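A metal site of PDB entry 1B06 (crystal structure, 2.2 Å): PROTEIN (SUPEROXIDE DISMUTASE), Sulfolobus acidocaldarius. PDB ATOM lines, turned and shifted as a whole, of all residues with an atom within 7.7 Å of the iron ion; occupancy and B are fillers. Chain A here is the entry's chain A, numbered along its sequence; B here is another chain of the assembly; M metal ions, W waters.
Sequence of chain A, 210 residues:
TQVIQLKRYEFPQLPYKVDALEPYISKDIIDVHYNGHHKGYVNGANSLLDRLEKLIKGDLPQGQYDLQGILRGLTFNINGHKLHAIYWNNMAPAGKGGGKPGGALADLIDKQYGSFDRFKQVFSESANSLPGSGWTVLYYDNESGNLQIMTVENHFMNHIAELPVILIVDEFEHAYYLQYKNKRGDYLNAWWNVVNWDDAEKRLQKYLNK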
ATOM      1  N   HIS A  33     -13.492  -2.892 -10.547  1.00  0.00           N
ATOM      2  CA  HIS A  33     -12.724  -1.810  -9.953  1.00  0.00           C
ATOM      3  C   HIS A  33     -13.337  -1.440  -8.603  1.00  0.00           C
ATOM      4  O   HIS A  33     -12.638  -1.193  -7.623  1.00  0.00           O
ATOM      5  CB  HIS A  33     -12.760  -0.578 -10.862  1.00  0.00           C
ATOM      6  CG  HIS A  33     -11.695   0.433 -10.568  1.00  0.00           C
ATOM      7  ND1 HIS A  33     -11.453   1.520 -11.396  1.00  0.00           N
ATOM      8  CD2 HIS A  33     -10.804   0.527  -9.558  1.00  0.00           C
ATOM      9  CE1 HIS A  33     -10.458   2.232 -10.899  1.00  0.00           C
ATOM     10  NE2 HIS A  33     -10.044   1.648  -9.784  1.00  0.00           N
ATOM     11  N   TYR A  34     -14.665  -1.413  -8.573  1.00  0.00           N
ATOM     12  CA  TYR A  34     -15.422  -1.070  -7.381  1.00  0.00           C
ATOM     13  C   TYR A  34     -15.637  -2.264  -6.446  1.00  0.00           C
ATOM     14  O   TYR A  34     -15.240  -2.224  -5.281  1.00  0.00           O
ATOM     15  CB  TYR A  34     -16.764  -0.463  -7.781  1.00  0.00           C
ATOM     16  CG  TYR A  34     -17.715  -0.233  -6.620  1.00  0.00           C
ATOM     17  CD1 TYR A  34     -17.468   0.750  -5.680  1.00  0.00           C
ATOM     18  CD2 TYR A  34     -18.836  -1.043  -6.455  1.00  0.00           C
ATOM     19  CE1 TYR A  34     -18.305   0.942  -4.589  1.00  0.00           C
ATOM     20  CE2 TYR A  34     -19.697  -0.865  -5.371  1.00  0.00           C
ATOM     21  CZ  TYR A  34     -19.418   0.123  -4.444  1.00  0.00           C
ATOM     22  OH  TYR A  34     -20.232   0.285  -3.346  1.00  0.00           O
ATOM     23  N   HIS A  37     -11.368  -4.298  -6.411  1.00  0.00           N
ATOM     24  CA  HIS A  37     -10.277  -3.514  -5.841  1.00  0.00           C
ATOM     25  C   HIS A  37     -10.630  -2.648  -4.628  1.00  0.00           C
ATOM     26  O   HIS A  37     -10.060  -2.821  -3.552  1.00  0.00           O
ATOM     27  CB  HIS A  37      -9.632  -2.653  -6.940  1.00  0.00           C
ATOM     28  CG  HIS A  37      -9.078  -3.452  -8.079  1.00  0.00           C
ATOM     29  ND1 HIS A  37      -7.830  -4.040  -8.034  1.00  0.00           N
ATOM     30  CD2 HIS A  37      -9.612  -3.781  -9.269  1.00  0.00           C
ATOM     31  CE1 HIS A  37      -7.622  -4.703  -9.157  1.00  0.00           C
ATOM     32  NE2 HIS A  37      -8.679  -4.559  -9.936  1.00  0.00           N
ATOM     33  N   HIS A  38     -11.578  -1.726  -4.780  1.00  0.00           N
ATOM     34  CA  HIS A  38     -11.939  -0.856  -3.666  1.00  0.00           C
ATOM     35  C   HIS A  38     -12.354  -1.652  -2.430  1.00  0.00           C
ATOM     36  O   HIS A  38     -11.872  -1.387  -1.333  1.00  0.00           O
ATOM     37  CB  HIS A  38     -13.061   0.103  -4.083  1.00  0.00           C
ATOM     38  CG  HIS A  38     -13.247   1.244  -3.135  1.00  0.00           C
ATOM     39  ND1 HIS A  38     -14.071   2.312  -3.406  1.00  0.00           N
ATOM     40  CD2 HIS A  38     -12.758   1.468  -1.890  1.00  0.00           C
ATOM     41  CE1 HIS A  38     -14.086   3.143  -2.385  1.00  0.00           C
ATOM     42  NE2 HIS A  38     -13.289   2.659  -1.449  1.00  0.00           N
ATOM     43  N   TYR A  41      -9.478  -2.975  -0.503  1.00  0.00           N
ATOM     44  CA  TYR A  41      -8.674  -2.032   0.268  1.00  0.00           C
ATOM     45  C   TYR A  41      -9.320  -1.793   1.624  1.00  0.00           C
ATOM     46  O   TYR A  41      -8.629  -1.603   2.618  1.00  0.00           O
ATOM     47  CB  TYR A  41      -8.533  -0.703  -0.490  1.00  0.00           C
ATOM     48  CG  TYR A  41      -7.734  -0.792  -1.780  1.00  0.00           C
ATOM     49  CD1 TYR A  41      -6.481  -1.433  -1.827  1.00  0.00           C
ATOM     50  CD2 TYR A  41      -8.224  -0.250  -2.974  1.00  0.00           C
ATOM     51  CE1 TYR A  41      -5.758  -1.528  -3.019  1.00  0.00           C
ATOM     52  CE2 TYR A  41      -7.501  -0.344  -4.166  1.00  0.00           C
ATOM     53  CZ  TYR A  41      -6.277  -0.976  -4.185  1.00  0.00           C
ATOM     54  OH  TYR A  41      -5.588  -1.075  -5.363  1.00  0.00           O
ATOM     55  N   GLY A  80      -5.634   3.637  -0.486  1.00  0.00           N
ATOM     56  CA  GLY A  80      -6.337   2.990  -1.580  1.00  0.00           C
ATOM     57  C   GLY A  80      -7.836   3.206  -1.481  1.00  0.00           C
ATOM     58  O   GLY A  80      -8.513   3.473  -2.473  1.00  0.00           O
ATOM     59  N   LEU A  83      -8.754   7.327  -1.646  1.00  0.00           N
ATOM     60  CA  LEU A  83      -8.566   7.878  -2.978  1.00  0.00           C
ATOM     61  C   LEU A  83      -9.632   7.379  -3.950  1.00  0.00           C
ATOM     62  O   LEU A  83     -10.079   8.128  -4.831  1.00  0.00           O
ATOM     63  CB  LEU A  83      -7.173   7.544  -3.510  1.00  0.00           C
ATOM     64  CG  LEU A  83      -6.006   8.242  -2.813  1.00  0.00           C
ATOM     65  CD1 LEU A  83      -4.726   7.910  -3.551  1.00  0.00           C
ATOM     66  CD2 LEU A  83      -6.230   9.744  -2.769  1.00  0.00           C
ATOM     67  N   HIS A  84     -10.046   6.122  -3.811  1.00  0.00           N
ATOM     68  CA  HIS A  84     -11.066   5.578  -4.697  1.00  0.00           C
ATOM     69  C   HIS A  84     -12.408   6.217  -4.368  1.00  0.00           C
ATOM     70  O   HIS A  84     -13.221   6.460  -5.256  1.00  0.00           O
ATOM     71  CB  HIS A  84     -11.156   4.058  -4.533  1.00  0.00           C
ATOM     72  CG  HIS A  84     -10.165   3.323  -5.383  1.00  0.00           C
ATOM     73  ND1 HIS A  84      -8.887   3.034  -4.955  1.00  0.00           N
ATOM     74  CD2 HIS A  84     -10.252   2.877  -6.651  1.00  0.00           C
ATOM     75  CE1 HIS A  84      -8.222   2.451  -5.937  1.00  0.00           C
ATOM     76  NE2 HIS A  84      -9.032   2.345  -6.974  1.00  0.00           N
ATOM     77  N   TYR A  87     -12.427   9.451  -6.128  1.00  0.00           N
ATOM     78  CA  TYR A  87     -12.472   9.157  -7.551  1.00  0.00           C
ATOM     79  C   TYR A  87     -13.898   8.929  -8.081  1.00  0.00           C
ATOM     80  O   TYR A  87     -14.288   9.526  -9.090  1.00  0.00           O
ATOM     81  CB  TYR A  87     -11.599   7.927  -7.817  1.00  0.00           C
ATOM     82  CG  TYR A  87     -11.499   7.466  -9.252  1.00  0.00           C
ATOM     83  CD1 TYR A  87     -11.096   8.331 -10.270  1.00  0.00           C
ATOM     84  CD2 TYR A  87     -11.749   6.144  -9.592  1.00  0.00           C
ATOM     85  CE1 TYR A  87     -10.941   7.881 -11.591  1.00  0.00           C
ATOM     86  CE2 TYR A  87     -11.599   5.680 -10.899  1.00  0.00           C
ATOM     87  CZ  TYR A  87     -11.194   6.552 -11.895  1.00  0.00           C
ATOM     88  OH  TYR A  87     -11.047   6.081 -13.181  1.00  0.00           O
ATOM     89  N   TRP A  88     -14.669   8.083  -7.409  1.00  0.00           N
ATOM     90  CA  TRP A  88     -16.040   7.799  -7.833  1.00  0.00           C
ATOM     91  C   TRP A  88     -16.891   9.054  -7.849  1.00  0.00           C
ATOM     92  O   TRP A  88     -17.668   9.278  -8.772  1.00  0.00           O
ATOM     93  CB  TRP A  88     -16.707   6.769  -6.919  1.00  0.00           C
ATOM     94  CG  TRP A  88     -15.954   5.478  -6.742  1.00  0.00           C
ATOM     95  CD1 TRP A  88     -15.721   4.827  -5.566  1.00  0.00           C
ATOM     96  CD2 TRP A  88     -15.339   4.681  -7.760  1.00  0.00           C
ATOM     97  NE1 TRP A  88     -15.012   3.674  -5.785  1.00  0.00           N
ATOM     98  CE2 TRP A  88     -14.759   3.556  -7.125  1.00  0.00           C
ATOM     99  CE3 TRP A  88     -15.220   4.794  -9.151  1.00  0.00           C
ATOM    100  CZ2 TRP A  88     -14.076   2.563  -7.825  1.00  0.00           C
ATOM    101  CZ3 TRP A  88     -14.538   3.794  -9.858  1.00  0.00           C
ATOM    102  CH2 TRP A  88     -13.971   2.695  -9.188  1.00  0.00           C
ATOM    103  N   GLY A 134      -0.287   4.569 -10.412  1.00  0.00           N
ATOM    104  CA  GLY A 134      -0.474   5.643  -9.457  1.00  0.00           C
ATOM    105  C   GLY A 134      -1.628   6.537  -9.818  1.00  0.00           C
ATOM    106  O   GLY A 134      -2.570   6.107 -10.483  1.00  0.00           O
ATOM    107  N   TRP A 135      -1.571   7.788  -9.368  1.00  0.00           N
ATOM    108  CA  TRP A 135      -2.629   8.755  -9.629  1.00  0.00           C
ATOM    109  C   TRP A 135      -2.030  10.116  -9.949  1.00  0.00           C
ATOM    110  O   TRP A 135      -0.871  10.388  -9.634  1.00  0.00           O
ATOM    111  CB  TRP A 135      -3.507   8.952  -8.389  1.00  0.00           C
ATOM    112  CG  TRP A 135      -3.992   7.729  -7.714  1.00  0.00           C
ATOM    113  CD1 TRP A 135      -3.243   6.801  -7.033  1.00  0.00           C
ATOM    114  CD2 TRP A 135      -5.356   7.298  -7.593  1.00  0.00           C
ATOM    115  NE1 TRP A 135      -4.051   5.835  -6.503  1.00  0.00           N
ATOM    116  CE2 TRP A 135      -5.357   6.109  -6.826  1.00  0.00           C
ATOM    117  CE3 TRP A 135      -6.572   7.805  -8.062  1.00  0.00           C
ATOM    118  CZ2 TRP A 135      -6.534   5.421  -6.519  1.00  0.00           C
ATOM    119  CZ3 TRP A 135      -7.750   7.117  -7.756  1.00  0.00           C
ATOM    120  CH2 TRP A 135      -7.718   5.932  -6.988  1.00  0.00           C
ATOM    121  N   HIS A 155      -0.370   4.229  -4.056  1.00  0.00           N
ATOM    122  CA  HIS A 155      -1.437   5.013  -3.426  1.00  0.00           C
ATOM    123  C   HIS A 155      -0.882   5.977  -2.376  1.00  0.00           C
ATOM    124  O   HIS A 155      -1.584   6.904  -1.959  1.00  0.00           O
ATOM    125  CB  HIS A 155      -2.434   4.092  -2.687  1.00  0.00           C
ATOM    126  CG  HIS A 155      -3.127   3.098  -3.569  1.00  0.00           C
ATOM    127  ND1 HIS A 155      -3.866   3.460  -4.675  1.00  0.00           N
ATOM    128  CD2 HIS A 155      -3.213   1.749  -3.482  1.00  0.00           C
ATOM    129  CE1 HIS A 155      -4.391   2.386  -5.223  1.00  0.00           C
ATOM    130  NE2 HIS A 155      -4.009   1.333  -4.527  1.00  0.00           N
ATOM    131  N   ASP A 170      -7.306   8.020 -11.587  1.00  0.00           N
ATOM    132  CA  ASP A 170      -6.670   6.766 -11.213  1.00  0.00           C
ATOM    133  C   ASP A 170      -5.857   6.307 -12.412  1.00  0.00           C
ATOM    134  O   ASP A 170      -6.396   6.254 -13.523  1.00  0.00           O
ATOM    135  CB  ASP A 170      -7.726   5.711 -10.878  1.00  0.00           C
ATOM    136  CG  ASP A 170      -7.138   4.450 -10.272  1.00  0.00           C
ATOM    137  OD1 ASP A 170      -5.899   4.281 -10.254  1.00  0.00           O
ATOM    138  OD2 ASP A 170      -7.945   3.617  -9.798  1.00  0.00           O
ATOM    139  N   GLU A 171      -4.587   5.986 -12.203  1.00  0.00           N
ATOM    140  CA  GLU A 171      -3.747   5.547 -13.303  1.00  0.00           C
ATOM    141  C   GLU A 171      -3.153   4.160 -13.100  1.00  0.00           C
ATOM    142  O   GLU A 171      -2.170   3.790 -13.758  1.00  0.00           O
ATOM    143  CB  GLU A 171      -2.639   6.570 -13.567  1.00  0.00           C
ATOM    144  CG  GLU A 171      -3.109   7.765 -14.398  1.00  0.00           C
ATOM    145  CD  GLU A 171      -1.973   8.675 -14.817  1.00  0.00           C
ATOM    146  OE1 GLU A 171      -1.275   8.357 -15.805  1.00  0.00           O
ATOM    147  OE2 GLU A 171      -1.770   9.705 -14.147  1.00  0.00           O
ATOM    148  N   PHE A 172      -3.731   3.398 -12.184  1.00  0.00           N
ATOM    149  CA  PHE A 172      -3.302   2.020 -11.969  1.00  0.00           C
ATOM    150  C   PHE A 172      -3.811   1.348 -13.237  1.00  0.00           C
ATOM    151  O   PHE A 172      -4.859   1.725 -13.760  1.00  0.00           O
ATOM    152  CB  PHE A 172      -4.012   1.418 -10.757  1.00  0.00           C
ATOM    153  CG  PHE A 172      -3.199   1.476  -9.494  1.00  0.00           C
ATOM    154  CD1 PHE A 172      -2.867   2.703  -8.920  1.00  0.00           C
ATOM    155  CD2 PHE A 172      -2.785   0.294  -8.868  1.00  0.00           C
ATOM    156  CE1 PHE A 172      -2.120   2.754  -7.728  1.00  0.00           C
ATOM    157  CE2 PHE A 172      -2.040   0.338  -7.684  1.00  0.00           C
ATOM    158  CZ  PHE A 172      -1.706   1.571  -7.117  1.00  0.00           C
ATOM    159  N   GLU A 173      -3.085   0.362 -13.745  1.00  0.00           N
ATOM    160  CA  GLU A 173      -3.512  -0.315 -14.977  1.00  0.00           C
ATOM    161  C   GLU A 173      -4.924  -0.894 -14.928  1.00  0.00           C
ATOM    162  O   GLU A 173      -5.593  -0.957 -15.949  1.00  0.00           O
ATOM    163  CB  GLU A 173      -2.496  -1.405 -15.347  1.00  0.00           C
ATOM    164  CG  GLU A 173      -1.168  -0.840 -15.778  1.00  0.00           C
ATOM    165  CD  GLU A 173      -0.123  -1.896 -15.978  1.00  0.00           C
ATOM    166  OE1 GLU A 173      -0.040  -2.830 -15.152  1.00  0.00           O
ATOM    167  OE2 GLU A 173       0.630  -1.794 -16.971  1.00  0.00           O
ATOM    168  N   HIS A 174      -5.372  -1.314 -13.741  1.00  0.00           N
ATOM    169  CA  HIS A 174      -6.703  -1.898 -13.599  1.00  0.00           C
ATOM    170  C   HIS A 174      -7.818  -0.882 -13.888  1.00  0.00           C
ATOM    171  O   HIS A 174      -8.979  -1.251 -14.083  1.00  0.00           O
ATOM    172  CB  HIS A 174      -6.885  -2.489 -12.203  1.00  0.00           C
ATOM    173  CG  HIS A 174      -6.954  -1.469 -11.105  1.00  0.00           C
ATOM    174  ND1 HIS A 174      -6.086  -1.472 -10.039  1.00  0.00           N
ATOM    175  CD2 HIS A 174      -7.823  -0.449 -10.882  1.00  0.00           C
ATOM    176  CE1 HIS A 174      -6.408  -0.494  -9.206  1.00  0.00           C
ATOM    177  NE2 HIS A 174      -7.457   0.137  -9.687  1.00  0.00           N
ATOM    178  N   ALA A 175      -7.462   0.393 -13.929  1.00  0.00           N
ATOM    179  CA  ALA A 175      -8.444   1.432 -14.181  1.00  0.00           C
ATOM    180  C   ALA A 175      -8.831   1.570 -15.657  1.00  0.00           C
ATOM    181  O   ALA A 175      -9.833   2.191 -15.975  1.00  0.00           O
ATOM    182  CB  ALA A 175      -7.930   2.762 -13.675  1.00  0.00           C
ATOM    183  N   TYR A 187      -7.009   6.605 -22.576  1.00  0.00           N
ATOM    184  CA  TYR A 187      -7.886   6.579 -21.408  1.00  0.00           C
ATOM    185  C   TYR A 187      -7.977   7.966 -20.776  1.00  0.00           C
ATOM    186  O   TYR A 187      -9.055   8.414 -20.416  1.00  0.00           O
ATOM    187  CB  TYR A 187      -7.352   5.555 -20.392  1.00  0.00           C
ATOM    188  CG  TYR A 187      -7.754   5.803 -18.947  1.00  0.00           C
ATOM    189  CD1 TYR A 187      -9.075   5.675 -18.535  1.00  0.00           C
ATOM    190  CD2 TYR A 187      -6.795   6.136 -17.985  1.00  0.00           C
ATOM    191  CE1 TYR A 187      -9.448   5.877 -17.197  1.00  0.00           C
ATOM    192  CE2 TYR A 187      -7.158   6.334 -16.646  1.00  0.00           C
ATOM    193  CZ  TYR A 187      -8.481   6.200 -16.255  1.00  0.00           C
ATOM    194  OH  TYR A 187      -8.833   6.403 -14.937  1.00  0.00           O
ATOM    195  N   GLU B 173       0.024  -5.337 -13.093  1.00  0.00           N
ATOM    196  CA  GLU B 173      -1.299  -5.793 -13.509  1.00  0.00           C
ATOM    197  C   GLU B 173      -1.369  -6.198 -14.989  1.00  0.00           C
ATOM    198  O   GLU B 173      -2.093  -7.134 -15.342  1.00  0.00           O
ATOM    199  CB  GLU B 173      -2.351  -4.721 -13.196  1.00  0.00           C
ATOM    200  CG  GLU B 173      -2.522  -4.505 -11.706  1.00  0.00           C
ATOM    201  CD  GLU B 173      -3.456  -3.360 -11.370  1.00  0.00           C
ATOM    202  OE1 GLU B 173      -3.371  -2.296 -12.017  1.00  0.00           O
ATOM    203  OE2 GLU B 173      -4.281  -3.527 -10.449  1.00  0.00           O
HETATM  204 FE    FE M   1      -8.029   1.986  -8.898  1.00  0.00          FE
HETATM  205  O   HOH W   1      -6.192   2.425  -8.029  1.00  0.00           O
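The side-chain carboxylate of Asp 170 is in hydrogen-bond range of the backbone NH of Phe 172 (3.0 Å).
O of His 33 sits at hydrogen-bond distance from N of His 38, at 3.1 Å.
The indole nitrogen (NE1) of Trp 88 sits close to the backbone carbonyl oxygen (O) of His 84 (3.4 Å).
A ring nitrogen (ND1) of His 84 is in hydrogen-bond range of the backbone carbonyl oxygen of Gly 80, at 2.5 Å.
The side-chain carboxylate (OE2) of Glu 173 of chain B lies within hydrogen-bond range of a ring nitrogen (ND1) of His 174, at 2.8 Å.
OH of Tyr 187 sits at hydrogen-bond distance from O of Asp 170.
Four residues have an atom within 4 Å of the iron ion: His 33, His 84, Asp 170 and His 174.
The iron ion is bound by the side-chain carboxylate of Asp 170 (1.9 Å), water W1 (2.1 Å), a ring nitrogen (NE2) of His 174 (2.1 Å), a ring nitrogen (NE2) of His 84 (2.2 Å) and a ring nitrogen (NE2) of His 33 (2.2 Å).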
